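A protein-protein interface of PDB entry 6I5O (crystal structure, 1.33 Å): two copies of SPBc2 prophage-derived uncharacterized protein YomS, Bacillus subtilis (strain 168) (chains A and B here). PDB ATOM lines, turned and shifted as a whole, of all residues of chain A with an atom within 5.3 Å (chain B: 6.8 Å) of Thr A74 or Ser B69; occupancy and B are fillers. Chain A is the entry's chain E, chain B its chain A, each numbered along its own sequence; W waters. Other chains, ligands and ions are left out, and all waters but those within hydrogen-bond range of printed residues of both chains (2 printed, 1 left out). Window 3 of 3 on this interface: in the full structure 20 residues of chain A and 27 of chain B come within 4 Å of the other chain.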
ATOM      1  N   ASN A  72     -22.113   6.503   3.278  1.00  0.00           N
ATOM      2  CA  ASN A  72     -21.540   6.548   4.640  1.00  0.00           C
ATOM      3  C   ASN A  72     -21.535   5.101   5.167  1.00  0.00           C
ATOM      4  O   ASN A  72     -22.594   4.484   5.233  1.00  0.00           O
ATOM      5  CB  ASN A  72     -22.394   7.510   5.456  1.00  0.00           C
ATOM      6  CG  ASN A  72     -21.929   7.722   6.871  1.00  0.00           C
ATOM      7  OD1 ASN A  72     -21.392   6.790   7.476  1.00  0.00           O
ATOM      8  ND2 ASN A  72     -22.235   8.889   7.411  1.00  0.00           N
ATOM      9  N   LYS A  73     -20.387   4.623   5.606  1.00  0.00           N
ATOM     10  CA  LYS A  73     -20.288   3.216   6.065  1.00  0.00           C
ATOM     11  C   LYS A  73     -20.934   2.989   7.430  1.00  0.00           C
ATOM     12  O   LYS A  73     -21.171   1.802   7.760  1.00  0.00           O
ATOM     13  CB  LYS A  73     -18.851   2.721   6.130  1.00  0.00           C
ATOM     14  CG  LYS A  73     -18.146   2.720   4.790  1.00  0.00           C
ATOM     15  CD  LYS A  73     -16.777   2.090   4.801  1.00  0.00           C
ATOM     16  CE  LYS A  73     -16.777   0.591   4.847  1.00  0.00           C
ATOM     17  NZ  LYS A  73     -17.211   0.062   3.535  1.00  0.00           N
ATOM     18  N   THR A  74     -21.298   4.050   8.158  1.00  0.00           N
ATOM     19  CA  THR A  74     -21.918   3.855   9.477  1.00  0.00           C
ATOM     20  C   THR A  74     -23.407   3.524   9.311  1.00  0.00           C
ATOM     21  O   THR A  74     -23.930   2.719  10.082  1.00  0.00           O
ATOM     22  CB  THR A  74     -21.713   5.078  10.366  1.00  0.00           C
ATOM     23  OG1 THR A  74     -20.333   5.112  10.728  1.00  0.00           O
ATOM     24  CG2 THR A  74     -22.545   5.040  11.615  1.00  0.00           C
ATOM     25  N   ASP A  75     -24.080   4.185   8.385  1.00  0.00           N
ATOM     26  CA  ASP A  75     -25.563   4.049   8.307  1.00  0.00           C
ATOM     27  C   ASP A  75     -26.073   3.859   6.884  1.00  0.00           C
ATOM     28  O   ASP A  75     -27.300   3.897   6.684  1.00  0.00           O
ATOM     29  CB  ASP A  75     -26.209   5.280   8.939  1.00  0.00           C
ATOM     30  CG  ASP A  75     -25.804   6.594   8.305  1.00  0.00           C
ATOM     31  OD1 ASP A  75     -25.136   6.604   7.213  1.00  0.00           O
ATOM     32  OD2 ASP A  75     -26.097   7.640   8.890  1.00  0.00           O
ATOM     33  N   PHE A  76     -25.195   3.682   5.919  1.00  0.00           N
ATOM     34  CA  PHE A  76     -25.518   3.509   4.480  1.00  0.00           C
ATOM     35  C   PHE A  76     -26.225   4.755   3.931  1.00  0.00           C
ATOM     36  O   PHE A  76     -26.810   4.631   2.874  1.00  0.00           O
ATOM     37  CB  PHE A  76     -26.302   2.220   4.259  1.00  0.00           C
ATOM     38  CG  PHE A  76     -25.522   0.965   4.497  1.00  0.00           C
ATOM     39  CD1 PHE A  76     -24.298   0.775   3.915  1.00  0.00           C
ATOM     40  CD2 PHE A  76     -25.939   0.024   5.413  1.00  0.00           C
ATOM     41  CE1 PHE A  76     -23.545  -0.366   4.174  1.00  0.00           C
ATOM     42  CE2 PHE A  76     -25.203  -1.128   5.646  1.00  0.00           C
ATOM     43  CZ  PHE A  76     -24.027  -1.338   4.999  1.00  0.00           C
ATOM     44  N   ASN A  86     -15.172  11.662  12.075  1.00  0.00           N
ATOM     45  CA  ASN A  86     -15.151  10.213  12.394  1.00  0.00           C
ATOM     46  C   ASN A  86     -16.155   9.468  11.507  1.00  0.00           C
ATOM     47  O   ASN A  86     -17.102   8.814  12.021  1.00  0.00           O
ATOM     48  CB  ASN A  86     -15.388   9.925  13.876  1.00  0.00           C
ATOM     49  CG  ASN A  86     -15.117   8.475  14.155  1.00  0.00           C
ATOM     50  OD1 ASN A  86     -14.400   7.800  13.431  1.00  0.00           O
ATOM     51  ND2 ASN A  86     -15.668   7.982  15.255  1.00  0.00           N
ATOM     52  N   TYR A  88     -16.443   7.244   7.567  1.00  0.00           N
ATOM     53  CA  TYR A  88     -15.978   6.668   6.285  1.00  0.00           C
ATOM     54  C   TYR A  88     -17.047   6.857   5.227  1.00  0.00           C
ATOM     55  O   TYR A  88     -18.201   6.565   5.443  1.00  0.00           O
ATOM     56  CB  TYR A  88     -15.718   5.168   6.410  1.00  0.00           C
ATOM     57  CG  TYR A  88     -14.592   4.778   7.303  1.00  0.00           C
ATOM     58  CD1 TYR A  88     -13.296   4.732   6.798  1.00  0.00           C
ATOM     59  CD2 TYR A  88     -14.789   4.487   8.640  1.00  0.00           C
ATOM     60  CE1 TYR A  88     -12.209   4.351   7.575  1.00  0.00           C
ATOM     61  CE2 TYR A  88     -13.724   4.093   9.427  1.00  0.00           C
ATOM     62  CZ  TYR A  88     -12.429   4.024   8.904  1.00  0.00           C
ATOM     63  OH  TYR A  88     -11.395   3.640   9.743  1.00  0.00           O
ATOM     64  N   PHE B  56     -19.978  -3.347  16.063  1.00  0.00           N
ATOM     65  CA  PHE B  56     -19.132  -3.557  14.886  1.00  0.00           C
ATOM     66  C   PHE B  56     -18.372  -2.278  14.596  1.00  0.00           C
ATOM     67  O   PHE B  56     -19.014  -1.206  14.545  1.00  0.00           O
ATOM     68  CB  PHE B  56     -19.993  -3.909  13.687  1.00  0.00           C
ATOM     69  CG  PHE B  56     -21.075  -4.945  13.872  1.00  0.00           C
ATOM     70  CD1 PHE B  56     -20.988  -5.928  14.842  1.00  0.00           C
ATOM     71  CD2 PHE B  56     -22.176  -4.948  13.038  1.00  0.00           C
ATOM     72  CE1 PHE B  56     -21.990  -6.881  14.944  1.00  0.00           C
ATOM     73  CE2 PHE B  56     -23.193  -5.892  13.154  1.00  0.00           C
ATOM     74  CZ  PHE B  56     -23.094  -6.843  14.126  1.00  0.00           C
ATOM     75  N   THR B  66     -14.978   3.602  14.493  1.00  0.00           N
ATOM     76  CA  THR B  66     -16.168   4.139  13.785  1.00  0.00           C
ATOM     77  C   THR B  66     -17.207   3.023  13.624  1.00  0.00           C
ATOM     78  O   THR B  66     -16.867   1.937  13.146  1.00  0.00           O
ATOM     79  CB  THR B  66     -15.810   4.639  12.392  1.00  0.00           C
ATOM     80  OG1 THR B  66     -14.626   5.426  12.415  1.00  0.00           O
ATOM     81  CG2 THR B  66     -16.942   5.447  11.789  1.00  0.00           C
ATOM     82  N   ALA B  67     -18.431   3.249  14.076  1.00  0.00           N
ATOM     83  CA  ALA B  67     -19.487   2.240  13.938  1.00  0.00           C
ATOM     84  C   ALA B  67     -19.598   1.806  12.464  1.00  0.00           C
ATOM     85  O   ALA B  67     -19.630   2.662  11.560  1.00  0.00           O
ATOM     86  CB  ALA B  67     -20.789   2.788  14.432  1.00  0.00           C
ATOM     87  N   LEU B  68     -19.665   0.509  12.245  1.00  0.00           N
ATOM     88  CA  LEU B  68     -19.595  -0.051  10.888  1.00  0.00           C
ATOM     89  C   LEU B  68     -20.851  -0.882  10.648  1.00  0.00           C
ATOM     90  O   LEU B  68     -21.079  -1.854  11.375  1.00  0.00           O
ATOM     91  CB  LEU B  68     -18.340  -0.916  10.787  1.00  0.00           C
ATOM     92  CG  LEU B  68     -18.139  -1.662   9.482  1.00  0.00           C
ATOM     93  CD1 LEU B  68     -17.946  -0.711   8.322  1.00  0.00           C
ATOM     94  CD2 LEU B  68     -16.998  -2.639   9.547  1.00  0.00           C
ATOM     95  N   SER B  69     -21.651  -0.512   9.657  1.00  0.00           N
ATOM     96  CA  SER B  69     -22.850  -1.320   9.301  1.00  0.00           C
ATOM     97  C   SER B  69     -22.479  -2.480   8.378  1.00  0.00           C
ATOM     98  O   SER B  69     -21.635  -2.351   7.486  1.00  0.00           O
ATOM     99  CB  SER B  69     -23.917  -0.453   8.705  1.00  0.00           C
ATOM    100  OG  SER B  69     -24.579   0.264   9.719  1.00  0.00           O
ATOM    101  N   GLY B  70     -23.172  -3.576   8.589  1.00  0.00           N
ATOM    102  CA  GLY B  70     -23.145  -4.756   7.730  1.00  0.00           C
ATOM    103  C   GLY B  70     -24.528  -5.294   7.557  1.00  0.00           C
ATOM    104  O   GLY B  70     -25.517  -4.669   7.997  1.00  0.00           O
ATOM    105  N   THR B  71     -24.566  -6.426   6.868  1.00  0.00           N
ATOM    106  CA  THR B  71     -25.833  -7.060   6.442  1.00  0.00           C
ATOM    107  C   THR B  71     -25.966  -8.425   7.098  1.00  0.00           C
ATOM    108  O   THR B  71     -25.065  -9.247   6.977  1.00  0.00           O
ATOM    109  CB  THR B  71     -25.934  -7.159   4.930  1.00  0.00           C
ATOM    110  OG1 THR B  71     -25.729  -5.840   4.377  1.00  0.00           O
ATOM    111  CG2 THR B  71     -27.256  -7.716   4.484  1.00  0.00           C
ATOM    112  N   LEU B  78     -29.884  -4.505   7.995  1.00  0.00           N
ATOM    113  CA  LEU B  78     -28.652  -3.728   8.146  1.00  0.00           C
ATOM    114  C   LEU B  78     -28.473  -3.406   9.614  1.00  0.00           C
ATOM    115  O   LEU B  78     -29.459  -3.166  10.324  1.00  0.00           O
ATOM    116  CB  LEU B  78     -28.754  -2.432   7.319  1.00  0.00           C
ATOM    117  CG  LEU B  78     -29.152  -2.669   5.867  1.00  0.00           C
ATOM    118  CD1 LEU B  78     -29.240  -1.355   5.119  1.00  0.00           C
ATOM    119  CD2 LEU B  78     -28.189  -3.602   5.198  1.00  0.00           C
ATOM    120  N   GLY B  79     -27.241  -3.353  10.052  1.00  0.00           N
ATOM    121  CA  GLY B  79     -26.980  -2.910  11.422  1.00  0.00           C
ATOM    122  C   GLY B  79     -25.504  -2.780  11.729  1.00  0.00           C
ATOM    123  O   GLY B  79     -24.685  -3.355  11.060  1.00  0.00           O
ATOM    124  N   SER B  80     -25.218  -2.029  12.780  1.00  0.00           N
ATOM    125  CA  SER B  80     -23.851  -1.806  13.274  1.00  0.00           C
ATOM    126  C   SER B  80     -23.665  -2.484  14.631  1.00  0.00           C
ATOM    127  O   SER B  80     -22.621  -2.274  15.239  1.00  0.00           O
ATOM    128  CB  SER B  80     -23.483  -0.355  13.332  1.00  0.00           C
ATOM    129  OG  SER B  80     -24.392   0.349  14.137  1.00  0.00           O
ATOM    130  N   SER B  81     -24.613  -3.288  15.064  1.00  0.00           N
ATOM    131  CA  SER B  81     -24.491  -4.011  16.350  1.00  0.00           C
ATOM    132  C   SER B  81     -25.497  -5.139  16.342  1.00  0.00           C
ATOM    133  O   SER B  81     -26.408  -5.140  15.513  1.00  0.00           O
ATOM    134  CB  SER B  81     -24.701  -3.111  17.526  1.00  0.00           C
ATOM    135  OG  SER B  81     -26.015  -2.558  17.537  1.00  0.00           O
ATOM    136  N   TRP B  89     -22.860 -11.853   9.734  1.00  0.00           N
ATOM    137  CA  TRP B  89     -22.943 -10.458   9.263  1.00  0.00           C
ATOM    138  C   TRP B  89     -21.874 -10.243   8.206  1.00  0.00           C
ATOM    139  O   TRP B  89     -20.686 -10.570   8.422  1.00  0.00           O
ATOM    140  CB  TRP B  89     -22.721  -9.498  10.420  1.00  0.00           C
ATOM    141  CG  TRP B  89     -23.844  -9.447  11.379  1.00  0.00           C
ATOM    142  CD1 TRP B  89     -24.036 -10.260  12.464  1.00  0.00           C
ATOM    143  CD2 TRP B  89     -24.948  -8.540  11.363  1.00  0.00           C
ATOM    144  NE1 TRP B  89     -25.208  -9.927  13.091  1.00  0.00           N
ATOM    145  CE2 TRP B  89     -25.781  -8.877  12.429  1.00  0.00           C
ATOM    146  CE3 TRP B  89     -25.314  -7.470  10.524  1.00  0.00           C
ATOM    147  CZ2 TRP B  89     -26.940  -8.168  12.732  1.00  0.00           C
ATOM    148  CZ3 TRP B  89     -26.472  -6.784  10.796  1.00  0.00           C
ATOM    149  CH2 TRP B  89     -27.250  -7.108  11.915  1.00  0.00           C
ATOM    150  N   ASP B  90     -22.275  -9.644   7.094  1.00  0.00           N
ATOM    151  CA  ASP B  90     -21.407  -9.377   5.928  1.00  0.00           C
ATOM    152  C   ASP B  90     -21.001  -7.905   5.881  1.00  0.00           C
ATOM    153  O   ASP B  90     -21.859  -7.028   6.071  1.00  0.00           O
ATOM    154  CB  ASP B  90     -22.123  -9.699   4.639  1.00  0.00           C
ATOM    155  CG  ASP B  90     -22.240 -11.138   4.293  1.00  0.00           C
ATOM    156  OD1 ASP B  90     -21.533 -11.975   4.930  1.00  0.00           O
ATOM    157  OD2 ASP B  90     -23.149 -11.409   3.459  1.00  0.00           O
ATOM    158  N   PHE B  91     -19.731  -7.685   5.588  1.00  0.00           N
ATOM    159  CA  PHE B  91     -19.168  -6.318   5.557  1.00  0.00           C
ATOM    160  C   PHE B  91     -18.301  -6.143   4.339  1.00  0.00           C
ATOM    161  O   PHE B  91     -17.574  -7.043   3.943  1.00  0.00           O
ATOM    162  CB  PHE B  91     -18.297  -6.036   6.779  1.00  0.00           C
ATOM    163  CG  PHE B  91     -18.994  -6.208   8.093  1.00  0.00           C
ATOM    164  CD1 PHE B  91     -19.090  -7.437   8.709  1.00  0.00           C
ATOM    165  CD2 PHE B  91     -19.642  -5.121   8.668  1.00  0.00           C
ATOM    166  CE1 PHE B  91     -19.763  -7.573   9.894  1.00  0.00           C
ATOM    167  CE2 PHE B  91     -20.314  -5.254   9.868  1.00  0.00           C
ATOM    168  CZ  PHE B  91     -20.384  -6.484  10.460  1.00  0.00           C
ATOM    169  N   ASP B  92     -18.378  -4.950   3.767  1.00  0.00           N
ATOM    170  CA  ASP B  92     -17.443  -4.492   2.721  1.00  0.00           C
ATOM    171  C   ASP B  92     -16.319  -3.735   3.418  1.00  0.00           C
ATOM    172  O   ASP B  92     -16.575  -2.683   4.026  1.00  0.00           O
ATOM    173  CB  ASP B  92     -18.141  -3.628   1.687  1.00  0.00           C
ATOM    174  CG  ASP B  92     -17.206  -3.019   0.652  1.00  0.00           C
ATOM    175  OD1 ASP B  92     -15.951  -3.276   0.609  1.00  0.00           O
ATOM    176  OD2 ASP B  92     -17.747  -2.243  -0.181  1.00  0.00           O
HETATM  177  O   HOH W   1     -12.082   4.704  12.196  1.00  0.00           O
HETATM  178  O   HOH W   2     -25.035   2.549  12.613  1.00  0.00           O
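OD1 of Asn A86 sits at hydrogen-bond distance from OG1 of Thr B66, 2.6 Å away. OG1 of Thr A74 sits at hydrogen-bond distance from O of Ala B67. The backbone NH (N) of Ser B69 is in hydrogen-bond range of the backbone carbonyl oxygen (O) of Lys A73, at 3.0 Å. The backbone carbonyl oxygen (O) of Thr A74 lies within hydrogen-bond range of the side-chain hydroxyl (OG) of Ser B69 (2.6 Å). The backbone carbonyl oxygen of Asp B92 lies within hydrogen-bond range of the side-chain amino group of Lys A73, at 2.9 Å.
Among the printed residues, pairs that only touch across the chains: Phe A76 with Ser B69 (3.4 Å), Tyr A88 with Thr B66 (3.4 Å), Thr A74 with Thr B66 (3.6 Å), Phe A76 with Leu B78 (3.6 Å) and Lys A73 with Leu B68 (3.9 Å).
Printed residues of chain B that touch a printed residue of chain A: Thr B66, Ala B67, Leu B68, Ser B69, Leu B78 and Asp B92. Hydrophobic or aromatic side chains of chain B that line the printed part of chain A: Leu B68 and Leu B78. Printed residues of chain A that touch a printed residue of chain B: Lys A73, Thr A74, Phe A76, Asn A86 and Tyr A88. Among the printed residues, 10 pairs touch across the chains. Among the printed residues, no Asp or Glu carboxylate lies within 4 Å of a Lys or Arg side-chain nitrogen of the other chain.
Water W1 bridges the side-chain hydroxyl of Thr B66 (2.7 Å) and the side-chain hydroxyl of Tyr A88 (2.8 Å). Water W2 lies within hydrogen-bond range of the side-chain hydroxyl (OG) of Ser B80 (2.8 Å) and the backbone carbonyl oxygen (O) of Thr A74 (2.8 Å).
Of the printed residues of chain B, Thr A74 touches Thr B66 (3.6 Å), Ala B67 (2.7 Å) and Ser B69 (2.6 Å). Of the printed residues of chain A, Leu B78 touches Phe A76. Of the printed residues of chain B, Phe A76 touches Ser B69 and Leu B78. Printed residues of chain A within 4 Å of Ala B67: Thr A74. Phe B56 touches none of the printed residues of chain A. The nearest printed residue of chain B that does not touch Thr A74 is Ser B80 (4.5 Å). The nearest printed residue of chain A that does not touch Ser B69 is Asp A75 (4.2 Å).
The backbone NH (N) of Leu B68 is in hydrogen-bond range of the backbone carbonyl oxygen (O) of Phe B56 (2.9 Å). The side-chain amide oxygen (OD1) of Asn A72 lies within hydrogen-bond range of the backbone NH (N) of Thr A74, 2.8 Å away. The backbone carbonyl oxygen (O) of Tyr A88 is in hydrogen-bond range of the backbone NH (N) of Lys A73, at 2.9 Å.
No position is printed for both chains. Of the 10 pairs that touch across the chains among the printed residues, none has its exchanged pair printed and touching as well.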
